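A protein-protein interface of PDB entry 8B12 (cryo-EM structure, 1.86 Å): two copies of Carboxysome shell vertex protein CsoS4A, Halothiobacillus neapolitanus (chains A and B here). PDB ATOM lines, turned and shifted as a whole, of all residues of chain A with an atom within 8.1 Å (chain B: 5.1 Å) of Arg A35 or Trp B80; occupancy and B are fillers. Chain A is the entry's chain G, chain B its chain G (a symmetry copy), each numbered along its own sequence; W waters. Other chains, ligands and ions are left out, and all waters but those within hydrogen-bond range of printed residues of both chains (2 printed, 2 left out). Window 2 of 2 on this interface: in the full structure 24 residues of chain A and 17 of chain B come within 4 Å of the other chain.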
ATOM      1  N   MET A   4      40.937  -6.448  18.235  1.00  0.00           N
ATOM      2  CA  MET A   4      39.937  -7.189  17.491  1.00  0.00           C
ATOM      3  C   MET A   4      40.347  -7.275  16.030  1.00  0.00           C
ATOM      4  O   MET A   4      41.089  -6.429  15.527  1.00  0.00           O
ATOM      5  CB  MET A   4      38.556  -6.537  17.617  1.00  0.00           C
ATOM      6  CG  MET A   4      37.989  -6.608  19.024  1.00  0.00           C
ATOM      7  SD  MET A   4      36.563  -5.548  19.276  1.00  0.00           S
ATOM      8  CE  MET A   4      35.283  -6.789  19.405  1.00  0.00           C
ATOM      9  N   GLU A   7      36.244  -8.446  10.411  1.00  0.00           N
ATOM     10  CA  GLU A   7      35.680  -9.568   9.670  1.00  0.00           C
ATOM     11  C   GLU A   7      35.078  -9.134   8.338  1.00  0.00           C
ATOM     12  O   GLU A   7      35.475  -9.636   7.283  1.00  0.00           O
ATOM     13  CB  GLU A   7      34.626 -10.286  10.520  1.00  0.00           C
ATOM     14  CG  GLU A   7      34.069 -11.525   9.856  1.00  0.00           C
ATOM     15  CD  GLU A   7      32.834 -12.050  10.546  1.00  0.00           C
ATOM     16  OE1 GLU A   7      32.675 -11.797  11.756  1.00  0.00           O
ATOM     17  OE2 GLU A   7      32.019 -12.716   9.875  1.00  0.00           O
ATOM     18  N   LYS A   8      34.129  -8.202   8.366  1.00  0.00           N
ATOM     19  CA  LYS A   8      33.425  -7.779   7.161  1.00  0.00           C
ATOM     20  C   LYS A   8      32.778  -6.427   7.427  1.00  0.00           C
ATOM     21  O   LYS A   8      32.828  -5.900   8.541  1.00  0.00           O
ATOM     22  CB  LYS A   8      32.388  -8.818   6.733  1.00  0.00           C
ATOM     23  CG  LYS A   8      31.479  -9.267   7.859  1.00  0.00           C
ATOM     24  CD  LYS A   8      30.402 -10.210   7.356  1.00  0.00           C
ATOM     25  CE  LYS A   8      29.530 -10.697   8.494  1.00  0.00           C
ATOM     26  NZ  LYS A   8      29.242 -12.149   8.372  1.00  0.00           N
ATOM     27  N   THR A   9      32.170  -5.866   6.389  1.00  0.00           N
ATOM     28  CA  THR A   9      31.487  -4.590   6.521  1.00  0.00           C
ATOM     29  C   THR A   9      30.056  -4.789   7.012  1.00  0.00           C
ATOM     30  O   THR A   9      29.481  -5.875   6.915  1.00  0.00           O
ATOM     31  CB  THR A   9      31.486  -3.837   5.188  1.00  0.00           C
ATOM     32  OG1 THR A   9      30.684  -4.546   4.237  1.00  0.00           O
ATOM     33  CG2 THR A   9      32.897  -3.710   4.651  1.00  0.00           C
ATOM     34  N   LEU A  10      29.485  -3.714   7.550  1.00  0.00           N
ATOM     35  CA  LEU A  10      28.117  -3.705   8.049  1.00  0.00           C
ATOM     36  C   LEU A  10      27.388  -2.516   7.440  1.00  0.00           C
ATOM     37  O   LEU A  10      27.901  -1.393   7.466  1.00  0.00           O
ATOM     38  CB  LEU A  10      28.096  -3.629   9.581  1.00  0.00           C
ATOM     39  CG  LEU A  10      26.840  -4.040  10.358  1.00  0.00           C
ATOM     40  CD1 LEU A  10      25.803  -2.927  10.379  1.00  0.00           C
ATOM     41  CD2 LEU A  10      26.252  -5.329   9.808  1.00  0.00           C
ATOM     42  N   VAL A  11      26.198  -2.760   6.893  1.00  0.00           N
ATOM     43  CA  VAL A  11      25.412  -1.736   6.218  1.00  0.00           C
ATOM     44  C   VAL A  11      24.032  -1.666   6.859  1.00  0.00           C
ATOM     45  O   VAL A  11      23.354  -2.690   6.999  1.00  0.00           O
ATOM     46  CB  VAL A  11      25.294  -2.012   4.708  1.00  0.00           C
ATOM     47  CG1 VAL A  11      24.297  -1.056   4.070  1.00  0.00           C
ATOM     48  CG2 VAL A  11      26.651  -1.895   4.042  1.00  0.00           C
ATOM     49  N   LEU A  25      32.071  -1.657  10.656  1.00  0.00           N
ATOM     50  CA  LEU A  25      32.744  -2.921  10.424  1.00  0.00           C
ATOM     51  C   LEU A  25      32.369  -3.915  11.515  1.00  0.00           C
ATOM     52  O   LEU A  25      32.149  -3.539  12.668  1.00  0.00           O
ATOM     53  CB  LEU A  25      34.266  -2.746  10.386  1.00  0.00           C
ATOM     54  CG  LEU A  25      34.843  -1.831   9.306  1.00  0.00           C
ATOM     55  CD1 LEU A  25      36.352  -1.738   9.436  1.00  0.00           C
ATOM     56  CD2 LEU A  25      34.446  -2.304   7.918  1.00  0.00           C
ATOM     57  N   VAL A  26      32.295  -5.185  11.139  1.00  0.00           N
ATOM     58  CA  VAL A  26      32.043  -6.260  12.089  1.00  0.00           C
ATOM     59  C   VAL A  26      33.385  -6.737  12.628  1.00  0.00           C
ATOM     60  O   VAL A  26      34.267  -7.133  11.860  1.00  0.00           O
ATOM     61  CB  VAL A  26      31.266  -7.414  11.439  1.00  0.00           C
ATOM     62  CG1 VAL A  26      31.036  -8.528  12.444  1.00  0.00           C
ATOM     63  CG2 VAL A  26      29.941  -6.916  10.881  1.00  0.00           C
ATOM     64  N   VAL A  27      33.539  -6.700  13.946  1.00  0.00           N
ATOM     65  CA  VAL A  27      34.793  -7.053  14.594  1.00  0.00           C
ATOM     66  C   VAL A  27      34.530  -8.137  15.627  1.00  0.00           C
ATOM     67  O   VAL A  27      33.465  -8.191  16.249  1.00  0.00           O
ATOM     68  CB  VAL A  27      35.468  -5.828  15.253  1.00  0.00           C
ATOM     69  CG1 VAL A  27      35.970  -4.865  14.199  1.00  0.00           C
ATOM     70  CG2 VAL A  27      34.502  -5.133  16.200  1.00  0.00           C
ATOM     71  N   TRP A  28      35.511  -9.019  15.791  1.00  0.00           N
ATOM     72  CA  TRP A  28      35.506 -10.005  16.858  1.00  0.00           C
ATOM     73  C   TRP A  28      36.936 -10.211  17.335  1.00  0.00           C
ATOM     74  O   TRP A  28      37.892  -9.990  16.591  1.00  0.00           O
ATOM     75  CB  TRP A  28      34.870 -11.338  16.420  1.00  0.00           C
ATOM     76  CG  TRP A  28      35.361 -11.898  15.113  1.00  0.00           C
ATOM     77  CD1 TRP A  28      36.504 -11.568  14.450  1.00  0.00           C
ATOM     78  CD2 TRP A  28      34.716 -12.905  14.322  1.00  0.00           C
ATOM     79  NE1 TRP A  28      36.607 -12.295  13.292  1.00  0.00           N
ATOM     80  CE2 TRP A  28      35.524 -13.126  13.191  1.00  0.00           C
ATOM     81  CE3 TRP A  28      33.535 -13.640  14.461  1.00  0.00           C
ATOM     82  CZ2 TRP A  28      35.189 -14.050  12.203  1.00  0.00           C
ATOM     83  CZ3 TRP A  28      33.204 -14.556  13.479  1.00  0.00           C
ATOM     84  CH2 TRP A  28      34.028 -14.752  12.366  1.00  0.00           C
ATOM     85  N   GLU A  29      37.073 -10.617  18.597  1.00  0.00           N
ATOM     86  CA  GLU A  29      38.405 -10.793  19.164  1.00  0.00           C
ATOM     87  C   GLU A  29      39.140 -11.961  18.518  1.00  0.00           C
ATOM     88  O   GLU A  29      40.371 -11.940  18.424  1.00  0.00           O
ATOM     89  CB  GLU A  29      38.312 -10.973  20.676  1.00  0.00           C
ATOM     90  CG  GLU A  29      38.282  -9.654  21.428  1.00  0.00           C
ATOM     91  CD  GLU A  29      37.938  -9.814  22.893  1.00  0.00           C
ATOM     92  OE1 GLU A  29      38.780  -9.452  23.741  1.00  0.00           O
ATOM     93  OE2 GLU A  29      36.825 -10.288  23.199  1.00  0.00           O
ATOM     94  N   LYS A  30      38.407 -12.973  18.067  1.00  0.00           N
ATOM     95  CA  LYS A  30      38.969 -14.074  17.300  1.00  0.00           C
ATOM     96  C   LYS A  30      37.840 -14.727  16.518  1.00  0.00           C
ATOM     97  O   LYS A  30      36.663 -14.516  16.834  1.00  0.00           O
ATOM     98  CB  LYS A  30      39.672 -15.095  18.214  1.00  0.00           C
ATOM     99  CG  LYS A  30      38.798 -16.245  18.685  1.00  0.00           C
ATOM    100  CD  LYS A  30      39.300 -16.805  20.010  1.00  0.00           C
ATOM    101  CE  LYS A  30      38.646 -16.123  21.201  1.00  0.00           C
ATOM    102  NZ  LYS A  30      37.161 -16.141  21.115  1.00  0.00           N
ATOM    103  N   PRO A  31      38.156 -15.482  15.468  1.00  0.00           N
ATOM    104  CA  PRO A  31      37.102 -16.207  14.748  1.00  0.00           C
ATOM    105  C   PRO A  31      36.328 -17.125  15.683  1.00  0.00           C
ATOM    106  O   PRO A  31      36.910 -17.890  16.454  1.00  0.00           O
ATOM    107  CB  PRO A  31      37.880 -16.995  13.688  1.00  0.00           C
ATOM    108  CG  PRO A  31      39.082 -16.158  13.437  1.00  0.00           C
ATOM    109  CD  PRO A  31      39.447 -15.551  14.763  1.00  0.00           C
ATOM    110  N   GLY A  32      35.001 -17.037  15.612  1.00  0.00           N
ATOM    111  CA  GLY A  32      34.125 -17.754  16.509  1.00  0.00           C
ATOM    112  C   GLY A  32      33.708 -16.987  17.746  1.00  0.00           C
ATOM    113  O   GLY A  32      32.749 -17.391  18.412  1.00  0.00           O
ATOM    114  N   ALA A  33      34.396 -15.895  18.071  1.00  0.00           N
ATOM    115  CA  ALA A  33      34.022 -15.072  19.207  1.00  0.00           C
ATOM    116  C   ALA A  33      32.757 -14.278  18.885  1.00  0.00           C
ATOM    117  O   ALA A  33      32.399 -14.117  17.717  1.00  0.00           O
ATOM    118  CB  ALA A  33      35.164 -14.128  19.573  1.00  0.00           C
ATOM    119  N   PRO A  34      32.053 -13.787  19.907  1.00  0.00           N
ATOM    120  CA  PRO A  34      30.862 -12.970  19.646  1.00  0.00           C
ATOM    121  C   PRO A  34      31.201 -11.750  18.802  1.00  0.00           C
ATOM    122  O   PRO A  34      32.232 -11.103  18.992  1.00  0.00           O
ATOM    123  CB  PRO A  34      30.388 -12.571  21.047  1.00  0.00           C
ATOM    124  CG  PRO A  34      30.933 -13.620  21.943  1.00  0.00           C
ATOM    125  CD  PRO A  34      32.235 -14.051  21.346  1.00  0.00           C
ATOM    126  N   ARG A  35      30.315 -11.440  17.860  1.00  0.00           N
ATOM    127  CA  ARG A  35      30.558 -10.351  16.928  1.00  0.00           C
ATOM    128  C   ARG A  35      30.131  -9.019  17.529  1.00  0.00           C
ATOM    129  O   ARG A  35      29.146  -8.938  18.264  1.00  0.00           O
ATOM    130  CB  ARG A  35      29.811 -10.591  15.618  1.00  0.00           C
ATOM    131  CG  ARG A  35      30.376 -11.714  14.778  1.00  0.00           C
ATOM    132  CD  ARG A  35      29.655 -11.816  13.449  1.00  0.00           C
ATOM    133  NE  ARG A  35      30.227 -12.847  12.595  1.00  0.00           N
ATOM    134  CZ  ARG A  35      29.648 -14.009  12.331  1.00  0.00           C
ATOM    135  NH1 ARG A  35      28.465 -14.320  12.834  1.00  0.00           N
ATOM    136  NH2 ARG A  35      30.269 -14.878  11.539  1.00  0.00           N
ATOM    137  N   GLN A  36      30.887  -7.976  17.208  1.00  0.00           N
ATOM    138  CA  GLN A  36      30.549  -6.611  17.571  1.00  0.00           C
ATOM    139  C   GLN A  36      30.720  -5.731  16.343  1.00  0.00           C
ATOM    140  O   GLN A  36      31.384  -6.105  15.375  1.00  0.00           O
ATOM    141  CB  GLN A  36      31.418  -6.095  18.728  1.00  0.00           C
ATOM    142  CG  GLN A  36      31.208  -6.834  20.040  1.00  0.00           C
ATOM    143  CD  GLN A  36      32.035  -6.264  21.172  1.00  0.00           C
ATOM    144  OE1 GLN A  36      31.828  -5.129  21.599  1.00  0.00           O
ATOM    145  NE2 GLN A  36      32.974  -7.053  21.671  1.00  0.00           N
ATOM    146  N   VAL A  37      30.091  -4.561  16.378  1.00  0.00           N
ATOM    147  CA  VAL A  37      30.143  -3.612  15.275  1.00  0.00           C
ATOM    148  C   VAL A  37      30.809  -2.341  15.775  1.00  0.00           C
ATOM    149  O   VAL A  37      30.380  -1.761  16.779  1.00  0.00           O
ATOM    150  CB  VAL A  37      28.742  -3.317  14.709  1.00  0.00           C
ATOM    151  CG1 VAL A  37      28.783  -2.115  13.779  1.00  0.00           C
ATOM    152  CG2 VAL A  37      28.203  -4.534  13.986  1.00  0.00           C
ATOM    153  N   ALA A  38      31.856  -1.913  15.080  1.00  0.00           N
ATOM    154  CA  ALA A  38      32.594  -0.717  15.444  1.00  0.00           C
ATOM    155  C   ALA A  38      32.486   0.320  14.338  1.00  0.00           C
ATOM    156  O   ALA A  38      32.316  -0.012  13.163  1.00  0.00           O
ATOM    157  CB  ALA A  38      34.068  -1.027  15.725  1.00  0.00           C
ATOM    158  N   LEU A  71      31.718   1.925  20.298  1.00  0.00           N
ATOM    159  CA  LEU A  71      32.848   1.111  19.861  1.00  0.00           C
ATOM    160  C   LEU A  71      33.391   1.721  18.577  1.00  0.00           C
ATOM    161  O   LEU A  71      32.713   1.701  17.546  1.00  0.00           O
ATOM    162  CB  LEU A  71      32.441  -0.343  19.645  1.00  0.00           C
ATOM    163  CG  LEU A  71      33.610  -1.310  19.453  1.00  0.00           C
ATOM    164  CD1 LEU A  71      34.475  -1.335  20.701  1.00  0.00           C
ATOM    165  CD2 LEU A  71      33.127  -2.701  19.102  1.00  0.00           C
ATOM    166  N   LYS B   2      26.429  -3.643  19.206  1.00  0.00           N
ATOM    167  CA  LYS B   2      26.138  -5.064  19.141  1.00  0.00           C
ATOM    168  C   LYS B   2      25.106  -5.342  18.059  1.00  0.00           C
ATOM    169  O   LYS B   2      24.385  -4.449  17.607  1.00  0.00           O
ATOM    170  CB  LYS B   2      25.631  -5.589  20.491  1.00  0.00           C
ATOM    171  CG  LYS B   2      26.427  -5.102  21.692  1.00  0.00           C
ATOM    172  CD  LYS B   2      27.228  -6.232  22.321  1.00  0.00           C
ATOM    173  CE  LYS B   2      27.680  -5.867  23.728  1.00  0.00           C
ATOM    174  NZ  LYS B   2      29.095  -5.408  23.760  1.00  0.00           N
ATOM    175  N   ILE B   3      25.056  -6.600  17.636  1.00  0.00           N
ATOM    176  CA  ILE B   3      24.063  -7.087  16.687  1.00  0.00           C
ATOM    177  C   ILE B   3      23.109  -7.988  17.452  1.00  0.00           C
ATOM    178  O   ILE B   3      23.517  -9.024  17.987  1.00  0.00           O
ATOM    179  CB  ILE B   3      24.714  -7.838  15.517  1.00  0.00           C
ATOM    180  CG1 ILE B   3      25.508  -6.873  14.637  1.00  0.00           C
ATOM    181  CG2 ILE B   3      23.663  -8.583  14.711  1.00  0.00           C
ATOM    182  CD1 ILE B   3      26.894  -7.369  14.296  1.00  0.00           C
ATOM    183  N   GLU B  29      21.095 -11.524  21.560  1.00  0.00           N
ATOM    184  CA  GLU B  29      22.052 -11.747  20.484  1.00  0.00           C
ATOM    185  C   GLU B  29      21.700 -12.982  19.665  1.00  0.00           C
ATOM    186  O   GLU B  29      21.992 -13.033  18.468  1.00  0.00           O
ATOM    187  CB  GLU B  29      23.465 -11.852  21.052  1.00  0.00           C
ATOM    188  CG  GLU B  29      24.134 -10.500  21.225  1.00  0.00           C
ATOM    189  CD  GLU B  29      25.423 -10.572  22.016  1.00  0.00           C
ATOM    190  OE1 GLU B  29      26.481 -10.219  21.454  1.00  0.00           O
ATOM    191  OE2 GLU B  29      25.380 -10.970  23.197  1.00  0.00           O
ATOM    192  N   TRP B  49      17.144  -8.026  12.700  1.00  0.00           N
ATOM    193  CA  TRP B  49      18.489  -7.905  13.242  1.00  0.00           C
ATOM    194  C   TRP B  49      18.860  -6.428  13.251  1.00  0.00           C
ATOM    195  O   TRP B  49      18.862  -5.780  12.199  1.00  0.00           O
ATOM    196  CB  TRP B  49      19.494  -8.713  12.422  1.00  0.00           C
ATOM    197  CG  TRP B  49      19.333 -10.190  12.555  1.00  0.00           C
ATOM    198  CD1 TRP B  49      18.666 -11.018  11.705  1.00  0.00           C
ATOM    199  CD2 TRP B  49      19.855 -11.022  13.597  1.00  0.00           C
ATOM    200  NE1 TRP B  49      18.735 -12.314  12.152  1.00  0.00           N
ATOM    201  CE2 TRP B  49      19.462 -12.343  13.312  1.00  0.00           C
ATOM    202  CE3 TRP B  49      20.617 -10.778  14.742  1.00  0.00           C
ATOM    203  CZ2 TRP B  49      19.803 -13.416  14.131  1.00  0.00           C
ATOM    204  CZ3 TRP B  49      20.955 -11.842  15.552  1.00  0.00           C
ATOM    205  CH2 TRP B  49      20.546 -13.146  15.244  1.00  0.00           C
ATOM    206  N   ILE B  77      19.802  -3.816  10.335  1.00  0.00           N
ATOM    207  CA  ILE B  77      20.775  -4.364   9.401  1.00  0.00           C
ATOM    208  C   ILE B  77      20.064  -4.796   8.128  1.00  0.00           C
ATOM    209  O   ILE B  77      19.062  -5.521   8.172  1.00  0.00           O
ATOM    210  CB  ILE B  77      21.536  -5.526  10.052  1.00  0.00           C
ATOM    211  CG1 ILE B  77      22.181  -5.046  11.354  1.00  0.00           C
ATOM    212  CG2 ILE B  77      22.577  -6.082   9.102  1.00  0.00           C
ATOM    213  CD1 ILE B  77      22.493  -6.152  12.323  1.00  0.00           C
ATOM    214  N   ASP B  78      20.578  -4.342   6.982  1.00  0.00           N
ATOM    215  CA  ASP B  78      19.926  -4.614   5.705  1.00  0.00           C
ATOM    216  C   ASP B  78      19.864  -6.111   5.423  1.00  0.00           C
ATOM    217  O   ASP B  78      18.831  -6.632   4.992  1.00  0.00           O
ATOM    218  CB  ASP B  78      20.657  -3.883   4.580  1.00  0.00           C
ATOM    219  CG  ASP B  78      20.331  -2.400   4.539  1.00  0.00           C
ATOM    220  OD1 ASP B  78      19.988  -1.836   5.598  1.00  0.00           O
ATOM    221  OD2 ASP B  78      20.430  -1.794   3.452  1.00  0.00           O
ATOM    222  N   GLN B  79      20.963  -6.822   5.671  1.00  0.00           N
ATOM    223  CA  GLN B  79      21.025  -8.260   5.435  1.00  0.00           C
ATOM    224  C   GLN B  79      21.904  -8.889   6.503  1.00  0.00           C
ATOM    225  O   GLN B  79      23.093  -8.574   6.594  1.00  0.00           O
ATOM    226  CB  GLN B  79      21.565  -8.566   4.034  1.00  0.00           C
ATOM    227  CG  GLN B  79      22.076  -9.986   3.852  1.00  0.00           C
ATOM    228  CD  GLN B  79      21.031 -10.913   3.253  1.00  0.00           C
ATOM    229  OE1 GLN B  79      19.922 -11.036   3.771  1.00  0.00           O
ATOM    230  NE2 GLN B  79      21.386 -11.568   2.153  1.00  0.00           N
ATOM    231  N   TRP B  80      21.319  -9.770   7.311  1.00  0.00           N
ATOM    232  CA  TRP B  80      22.057 -10.458   8.360  1.00  0.00           C
ATOM    233  C   TRP B  80      21.460 -11.840   8.561  1.00  0.00           C
ATOM    234  O   TRP B  80      20.243 -12.017   8.481  1.00  0.00           O
ATOM    235  CB  TRP B  80      22.028  -9.674   9.676  1.00  0.00           C
ATOM    236  CG  TRP B  80      22.911 -10.257  10.727  1.00  0.00           C
ATOM    237  CD1 TRP B  80      22.537 -11.081  11.745  1.00  0.00           C
ATOM    238  CD2 TRP B  80      24.323 -10.072  10.859  1.00  0.00           C
ATOM    239  NE1 TRP B  80      23.627 -11.418  12.504  1.00  0.00           N
ATOM    240  CE2 TRP B  80      24.736 -10.811  11.982  1.00  0.00           C
ATOM    241  CE3 TRP B  80      25.277  -9.349  10.138  1.00  0.00           C
ATOM    242  CZ2 TRP B  80      26.060 -10.850  12.402  1.00  0.00           C
ATOM    243  CZ3 TRP B  80      26.591  -9.387  10.558  1.00  0.00           C
ATOM    244  CH2 TRP B  80      26.973 -10.134  11.677  1.00  0.00           C
ATOM    245  N   ASN B  81      22.322 -12.816   8.822  1.00  0.00           N
ATOM    246  CA  ASN B  81      21.872 -14.180   9.078  1.00  0.00           C
ATOM    247  C   ASN B  81      21.810 -14.456  10.576  1.00  0.00           C
ATOM    248  O   ASN B  81      22.784 -14.242  11.295  1.00  0.00           O
ATOM    249  CB  ASN B  81      22.795 -15.189   8.394  1.00  0.00           C
ATOM    250  CG  ASN B  81      22.523 -15.313   6.906  1.00  0.00           C
ATOM    251  OD1 ASN B  81      21.373 -15.403   6.478  1.00  0.00           O
ATOM    252  ND2 ASN B  81      23.585 -15.326   6.110  1.00  0.00           N
HETATM  253  O   HOH W   1      30.081  -3.257  21.338  1.00  0.00           O
HETATM  254  O   HOH W   2      23.617  -5.467   5.599  1.00  0.00           O
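Water W1 bridges the side-chain amide oxygen of Gln A36 and the side-chain amino group of Lys B2. Water W2 lies within hydrogen-bond range of the backbone NH (N) of Gln B79 (3.0 Å) and the backbone carbonyl oxygen (O) of Val A11 (3.1 Å).
Trp B80 touches Lys A8. CD2 of Leu A10 touches CG2 of Ile B77, at 3.8 Å. CA of Ile B77 touches O of Val A11 (3.9 Å). Arg A35 touches Trp B80. CG2 of Val A37 touches CD1 of Ile B3, 3.1 Å away.
Of the printed residues of chain B, Lys A8 touches Trp B80. Printed residues of chain B within 4 Å of Leu A10: Ile B77 (3.8 Å). Pro A31 touches none of the printed residues of chain B. Arg A35 touches one residue of chain B. Printed residues of chain B within 4 Å of Gln A36: Lys B2 (3.5 Å). Printed residues of chain B within 4 Å of Val A37: Ile B3. Printed residues of chain A within 4 Å of Ile B77: Leu A10 and Val A11. The nearest residue of chain B that does not touch Arg A35 is Glu B29 (4.3 Å). The nearest residue of chain A that does not touch Trp B80 is Leu A10 (4.1 Å).
Among the printed residues, 7 pairs touch across the chains. Among the printed residues, no Asp or Glu carboxylate lies within 4 Å of a Lys or Arg side-chain nitrogen of the other chain.
O of Lys A8 sits at hydrogen-bond distance from N of Val A26 (2.7 Å). The side-chain carboxylate of Glu A7 lies within salt-bridge range of the guanidinium group of Arg A35 (2.8 Å). The side-chain carboxylate (OE2) of Glu A7 lies within salt-bridge range of the side-chain amino group (NZ) of Lys A8 (3.2 Å). The backbone NH of Ile B77 lies within hydrogen-bond range of the backbone carbonyl oxygen of Trp B49 (2.9 Å). N of Val A27 is in hydrogen-bond range of O of Gln A36 (2.7 Å).
NZ of Lys B2 is in hydrogen-bond range of OE1 of Gln A36. The backbone carbonyl oxygen (O) of Val A11 lies within hydrogen-bond range of the backbone NH (N) of Asp B78 (3.2 Å).
1 position is printed for both chains.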
